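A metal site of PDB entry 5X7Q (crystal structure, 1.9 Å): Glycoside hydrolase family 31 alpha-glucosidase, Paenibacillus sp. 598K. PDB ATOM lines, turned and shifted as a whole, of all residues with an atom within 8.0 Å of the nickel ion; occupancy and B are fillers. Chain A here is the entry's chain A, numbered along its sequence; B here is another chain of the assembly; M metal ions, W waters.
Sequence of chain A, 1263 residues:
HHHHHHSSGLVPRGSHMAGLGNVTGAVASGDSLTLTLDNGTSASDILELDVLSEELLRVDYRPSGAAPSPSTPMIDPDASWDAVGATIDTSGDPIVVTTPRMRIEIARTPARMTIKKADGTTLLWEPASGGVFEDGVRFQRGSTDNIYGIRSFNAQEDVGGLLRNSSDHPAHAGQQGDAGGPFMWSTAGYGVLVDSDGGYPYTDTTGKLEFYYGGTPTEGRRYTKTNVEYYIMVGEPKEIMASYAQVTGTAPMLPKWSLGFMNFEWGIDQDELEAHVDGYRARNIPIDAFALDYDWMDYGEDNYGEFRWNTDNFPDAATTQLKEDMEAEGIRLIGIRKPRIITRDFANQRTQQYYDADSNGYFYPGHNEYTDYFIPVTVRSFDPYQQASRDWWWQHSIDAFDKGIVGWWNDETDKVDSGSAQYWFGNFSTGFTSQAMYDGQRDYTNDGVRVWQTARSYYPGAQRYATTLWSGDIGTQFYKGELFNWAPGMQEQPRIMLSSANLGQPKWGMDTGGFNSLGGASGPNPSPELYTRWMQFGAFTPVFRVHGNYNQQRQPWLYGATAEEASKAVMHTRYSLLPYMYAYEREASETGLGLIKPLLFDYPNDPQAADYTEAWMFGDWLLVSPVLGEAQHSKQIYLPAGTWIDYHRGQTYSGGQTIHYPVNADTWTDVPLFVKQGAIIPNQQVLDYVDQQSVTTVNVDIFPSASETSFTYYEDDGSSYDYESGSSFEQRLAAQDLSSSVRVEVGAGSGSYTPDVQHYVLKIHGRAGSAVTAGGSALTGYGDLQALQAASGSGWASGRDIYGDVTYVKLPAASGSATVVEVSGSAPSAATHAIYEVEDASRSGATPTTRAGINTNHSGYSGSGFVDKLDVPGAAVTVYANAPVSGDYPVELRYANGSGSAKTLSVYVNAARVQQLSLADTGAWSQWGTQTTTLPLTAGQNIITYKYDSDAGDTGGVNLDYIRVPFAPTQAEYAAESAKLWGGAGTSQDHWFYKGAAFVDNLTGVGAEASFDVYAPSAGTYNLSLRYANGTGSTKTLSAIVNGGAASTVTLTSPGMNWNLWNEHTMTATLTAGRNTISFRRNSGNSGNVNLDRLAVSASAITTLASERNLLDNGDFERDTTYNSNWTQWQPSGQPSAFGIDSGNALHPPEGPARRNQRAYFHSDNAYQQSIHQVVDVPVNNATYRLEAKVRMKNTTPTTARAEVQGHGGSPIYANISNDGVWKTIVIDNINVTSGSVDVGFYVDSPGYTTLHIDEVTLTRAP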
ATOM      1  N   ILE A 150     -14.099  -1.318 -10.031  1.00  0.00           N
ATOM      2  CA  ILE A 150     -15.564  -1.230 -10.187  1.00  0.00           C
ATOM      3  C   ILE A 150     -16.341  -2.140  -9.233  1.00  0.00           C
ATOM      4  O   ILE A 150     -17.235  -1.679  -8.516  1.00  0.00           O
ATOM      5  CB  ILE A 150     -16.029  -1.476 -11.638  1.00  0.00           C
ATOM      6  CG1 ILE A 150     -15.536  -0.356 -12.570  1.00  0.00           C
ATOM      7  CG2 ILE A 150     -17.546  -1.568 -11.727  1.00  0.00           C
ATOM      8  CD1 ILE A 150     -15.594  -0.700 -14.052  1.00  0.00           C
ATOM      9  N   ARG A 151     -16.030  -3.428  -9.260  1.00  0.00           N
ATOM     10  CA  ARG A 151     -16.895  -4.435  -8.644  1.00  0.00           C
ATOM     11  C   ARG A 151     -16.133  -5.705  -8.332  1.00  0.00           C
ATOM     12  O   ARG A 151     -15.087  -5.981  -8.934  1.00  0.00           O
ATOM     13  CB  ARG A 151     -18.083  -4.770  -9.556  1.00  0.00           C
ATOM     14  CG  ARG A 151     -17.752  -5.283 -10.961  1.00  0.00           C
ATOM     15  CD  ARG A 151     -17.645  -6.804 -11.076  1.00  0.00           C
ATOM     16  NE  ARG A 151     -18.862  -7.474 -10.635  1.00  0.00           N
ATOM     17  CZ  ARG A 151     -19.886  -7.824 -11.407  1.00  0.00           C
ATOM     18  NH1 ARG A 151     -19.899  -7.587 -12.715  1.00  0.00           N
ATOM     19  NH2 ARG A 151     -20.932  -8.431 -10.861  1.00  0.00           N
ATOM     20  N   SER A 152     -16.702  -6.484  -7.405  1.00  0.00           N
ATOM     21  CA  SER A 152     -16.291  -7.852  -7.126  1.00  0.00           C
ATOM     22  C   SER A 152     -17.528  -8.744  -7.298  1.00  0.00           C
ATOM     23  O   SER A 152     -18.443  -8.409  -8.063  1.00  0.00           O
ATOM     24  CB  SER A 152     -15.751  -7.904  -5.702  1.00  0.00           C
ATOM     25  OG  SER A 152     -15.233  -9.187  -5.401  1.00  0.00           O
ATOM     26  N   PHE A 153     -17.569  -9.879  -6.601  1.00  0.00           N
ATOM     27  CA  PHE A 153     -18.672 -10.833  -6.719  1.00  0.00           C
ATOM     28  C   PHE A 153     -19.109 -11.300  -5.352  1.00  0.00           C
ATOM     29  O   PHE A 153     -18.284 -11.474  -4.443  1.00  0.00           O
ATOM     30  CB  PHE A 153     -18.249 -11.992  -7.612  1.00  0.00           C
ATOM     31  CG  PHE A 153     -17.667 -11.554  -8.906  1.00  0.00           C
ATOM     32  CD1 PHE A 153     -18.505 -11.219  -9.978  1.00  0.00           C
ATOM     33  CD2 PHE A 153     -16.284 -11.381  -9.045  1.00  0.00           C
ATOM     34  CE1 PHE A 153     -17.970 -10.750 -11.177  1.00  0.00           C
ATOM     35  CE2 PHE A 153     -15.762 -10.923 -10.239  1.00  0.00           C
ATOM     36  CZ  PHE A 153     -16.603 -10.606 -11.298  1.00  0.00           C
ATOM     37  N   ASN A 154     -20.411 -11.492  -5.185  1.00  0.00           N
ATOM     38  CA  ASN A 154     -20.965 -11.868  -3.888  1.00  0.00           C
ATOM     39  C   ASN A 154     -21.191 -13.380  -3.799  1.00  0.00           C
ATOM     40  O   ASN A 154     -20.998 -14.088  -4.782  1.00  0.00           O
ATOM     41  CB  ASN A 154     -22.224 -11.053  -3.533  1.00  0.00           C
ATOM     42  CG  ASN A 154     -23.459 -11.404  -4.353  1.00  0.00           C
ATOM     43  OD1 ASN A 154     -23.657 -12.540  -4.832  1.00  0.00           O
ATOM     44  ND2 ASN A 154     -24.341 -10.419  -4.466  1.00  0.00           N
ATOM     45  N   GLU A 157     -23.598 -14.998  -6.550  1.00  0.00           N
ATOM     46  CA  GLU A 157     -23.371 -14.608  -7.939  1.00  0.00           C
ATOM     47  C   GLU A 157     -22.456 -15.586  -8.628  1.00  0.00           C
ATOM     48  O   GLU A 157     -21.639 -16.249  -7.988  1.00  0.00           O
ATOM     49  CB  GLU A 157     -22.739 -13.216  -8.003  1.00  0.00           C
ATOM     50  CG  GLU A 157     -23.771 -12.106  -7.961  1.00  0.00           C
ATOM     51  CD  GLU A 157     -23.195 -10.708  -7.863  1.00  0.00           C
ATOM     52  OE1 GLU A 157     -22.025 -10.519  -7.405  1.00  0.00           O
ATOM     53  OE2 GLU A 157     -23.949  -9.785  -8.223  1.00  0.00           O
ATOM     54  N   HIS A 169     -21.938  -2.971 -14.673  1.00  0.00           N
ATOM     55  CA  HIS A 169     -22.403  -3.263 -13.322  1.00  0.00           C
ATOM     56  C   HIS A 169     -22.329  -1.964 -12.504  1.00  0.00           C
ATOM     57  O   HIS A 169     -21.370  -1.219 -12.687  1.00  0.00           O
ATOM     58  CB  HIS A 169     -21.499  -4.332 -12.714  1.00  0.00           C
ATOM     59  CG  HIS A 169     -22.049  -4.979 -11.491  1.00  0.00           C
ATOM     60  ND1 HIS A 169     -23.076  -5.907 -11.532  1.00  0.00           N
ATOM     61  CD2 HIS A 169     -21.678  -4.886 -10.180  1.00  0.00           C
ATOM     62  CE1 HIS A 169     -23.342  -6.310 -10.302  1.00  0.00           C
ATOM     63  NE2 HIS A 169     -22.499  -5.720  -9.473  1.00  0.00           N
ATOM     64  N   PRO A 170     -23.316  -1.672 -11.635  1.00  0.00           N
ATOM     65  CA  PRO A 170     -23.200  -0.449 -10.812  1.00  0.00           C
ATOM     66  C   PRO A 170     -22.062  -0.491  -9.807  1.00  0.00           C
ATOM     67  O   PRO A 170     -21.580  -1.576  -9.453  1.00  0.00           O
ATOM     68  CB  PRO A 170     -24.538  -0.385 -10.061  1.00  0.00           C
ATOM     69  CG  PRO A 170     -25.437  -1.370 -10.704  1.00  0.00           C
ATOM     70  CD  PRO A 170     -24.562  -2.395 -11.354  1.00  0.00           C
ATOM     71  N   ALA A 171     -21.654   0.706  -9.361  1.00  0.00           N
ATOM     72  CA  ALA A 171     -20.714   0.866  -8.264  1.00  0.00           C
ATOM     73  C   ALA A 171     -21.510   0.871  -6.972  1.00  0.00           C
ATOM     74  O   ALA A 171     -22.308   1.778  -6.732  1.00  0.00           O
ATOM     75  CB  ALA A 171     -19.906   2.164  -8.405  1.00  0.00           C
ATOM     76  N   HIS A 172     -21.299  -0.145  -6.144  1.00  0.00           N
ATOM     77  CA  HIS A 172     -21.984  -0.262  -4.869  1.00  0.00           C
ATOM     78  C   HIS A 172     -21.186  -1.115  -3.877  1.00  0.00           C
ATOM     79  O   HIS A 172     -20.331  -1.908  -4.279  1.00  0.00           O
ATOM     80  CB  HIS A 172     -23.401  -0.844  -5.059  1.00  0.00           C
ATOM     81  CG  HIS A 172     -23.458  -2.147  -5.798  1.00  0.00           C
ATOM     82  ND1 HIS A 172     -24.413  -2.408  -6.758  1.00  0.00           N
ATOM     83  CD2 HIS A 172     -22.736  -3.304  -5.678  1.00  0.00           C
ATOM     84  CE1 HIS A 172     -24.250  -3.637  -7.232  1.00  0.00           C
ATOM     85  NE2 HIS A 172     -23.240  -4.199  -6.581  1.00  0.00           N
ATOM     86  N   ALA A 173     -21.497  -0.958  -2.594  1.00  0.00           N
ATOM     87  CA  ALA A 173     -21.022  -1.871  -1.553  1.00  0.00           C
ATOM     88  C   ALA A 173     -21.569  -3.274  -1.780  1.00  0.00           C
ATOM     89  O   ALA A 173     -20.843  -4.250  -1.579  1.00  0.00           O
ATOM     90  CB  ALA A 173     -21.444  -1.377  -0.188  1.00  0.00           C
ATOM     91  N   GLY A 174     -22.834  -3.371  -2.179  1.00  0.00           N
ATOM     92  CA  GLY A 174     -23.501  -4.666  -2.443  1.00  0.00           C
ATOM     93  C   GLY A 174     -23.777  -5.436  -1.159  1.00  0.00           C
ATOM     94  O   GLY A 174     -23.912  -4.860  -0.086  1.00  0.00           O
ATOM     95  N   GLN A 175     -23.859  -6.766  -1.291  1.00  0.00           N
ATOM     96  CA  GLN A 175     -24.137  -7.653  -0.155  1.00  0.00           C
ATOM     97  C   GLN A 175     -23.309  -8.934  -0.226  1.00  0.00           C
ATOM     98  O   GLN A 175     -22.709  -9.224  -1.256  1.00  0.00           O
ATOM     99  CB  GLN A 175     -25.623  -8.025  -0.114  1.00  0.00           C
ATOM    100  CG  GLN A 175     -26.097  -8.772  -1.345  1.00  0.00           C
ATOM    101  CD  GLN A 175     -27.471  -9.384  -1.203  1.00  0.00           C
ATOM    102  OE1 GLN A 175     -27.838  -9.950  -0.154  1.00  0.00           O
ATOM    103  NE2 GLN A 175     -28.254  -9.277  -2.264  1.00  0.00           N
ATOM    104  N   GLY A 177     -20.427 -10.314   0.661  1.00  0.00           N
ATOM    105  CA  GLY A 177     -19.017 -10.380   0.261  1.00  0.00           C
ATOM    106  C   GLY A 177     -18.634  -9.514  -0.916  1.00  0.00           C
ATOM    107  O   GLY A 177     -17.457  -9.458  -1.273  1.00  0.00           O
ATOM    108  N   ASP A 178     -19.606  -8.799  -1.479  1.00  0.00           N
ATOM    109  CA  ASP A 178     -19.356  -7.906  -2.590  1.00  0.00           C
ATOM    110  C   ASP A 178     -18.523  -6.713  -2.143  1.00  0.00           C
ATOM    111  O   ASP A 178     -18.389  -6.410  -0.957  1.00  0.00           O
ATOM    112  CB  ASP A 178     -20.688  -7.405  -3.170  1.00  0.00           C
ATOM    113  CG  ASP A 178     -20.633  -7.089  -4.648  1.00  0.00           C
ATOM    114  OD1 ASP A 178     -19.544  -7.079  -5.267  1.00  0.00           O
ATOM    115  OD2 ASP A 178     -21.746  -6.838  -5.185  1.00  0.00           O
ATOM    116  N   ALA A 179     -17.953  -6.065  -3.133  1.00  0.00           N
ATOM    117  CA  ALA A 179     -17.209  -4.842  -2.952  1.00  0.00           C
ATOM    118  C   ALA A 179     -17.369  -4.102  -4.257  1.00  0.00           C
ATOM    119  O   ALA A 179     -17.573  -4.713  -5.313  1.00  0.00           O
ATOM    120  CB  ALA A 179     -15.757  -5.141  -2.675  1.00  0.00           C
ATOM    121  N   GLY A 180     -17.275  -2.786  -4.189  1.00  0.00           N
ATOM    122  CA  GLY A 180     -17.327  -1.988  -5.386  1.00  0.00           C
ATOM    123  C   GLY A 180     -17.144  -0.527  -5.102  1.00  0.00           C
ATOM    124  O   GLY A 180     -17.052  -0.100  -3.940  1.00  0.00           O
ATOM    125  N   TRP B 424     -32.412  -2.494   1.772  1.00  0.00           N
ATOM    126  CA  TRP B 424     -31.004  -2.266   1.528  1.00  0.00           C
ATOM    127  C   TRP B 424     -30.440  -1.246   2.494  1.00  0.00           C
ATOM    128  O   TRP B 424     -31.095  -0.246   2.785  1.00  0.00           O
ATOM    129  CB  TRP B 424     -30.789  -1.759   0.112  1.00  0.00           C
ATOM    130  CG  TRP B 424     -30.746  -2.824  -0.900  1.00  0.00           C
ATOM    131  CD1 TRP B 424     -31.792  -3.314  -1.627  1.00  0.00           C
ATOM    132  CD2 TRP B 424     -29.581  -3.542  -1.309  1.00  0.00           C
ATOM    133  NE1 TRP B 424     -31.337  -4.290  -2.481  1.00  0.00           N
ATOM    134  CE2 TRP B 424     -29.986  -4.464  -2.301  1.00  0.00           C
ATOM    135  CE3 TRP B 424     -28.227  -3.495  -0.933  1.00  0.00           C
ATOM    136  CZ2 TRP B 424     -29.091  -5.343  -2.923  1.00  0.00           C
ATOM    137  CZ3 TRP B 424     -27.338  -4.364  -1.549  1.00  0.00           C
ATOM    138  CH2 TRP B 424     -27.773  -5.283  -2.530  1.00  0.00           C
HETATM  139 NI    NI M   1     -22.116  -6.168  -7.236  1.00  0.00          NI
HETATM  140  O   HOH W   1     -20.148  -5.091  -7.097  1.00  0.00           O
HETATM  141  O   HOH W   2     -21.199  -8.094  -7.891  1.00  0.00           O
HETATM  142  O   HOH W   3     -23.936  -7.394  -7.243  1.00  0.00           O
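ND1 of His 169 lies close to NH2 of Arg 151 (3.4 Å).
The backbone NH of Gly 180 sits at hydrogen-bond distance from the backbone carbonyl oxygen of His 172.
OD2 of Asp 178 is bound to the nickel ion, 2.2 Å away.
Water W3 binds the nickel ion (2.2 Å).
Water W2 is bound to the nickel ion (2.2 Å).
The nickel ion is bound by water W1, 2.2 Å away.
NE2 of His 169 binds the nickel ion.
NE2 of His 172 is bound to the nickel ion (2.4 Å).
Of the 18 residues printed, 3 come within 4 Å of the nickel ion.
The nearest printed residue that does not touch the nickel ion is Glu 157 (4.2 Å).
Water W1 lies within hydrogen-bond range of OD1 of Asp 178 and O of Ala 179.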
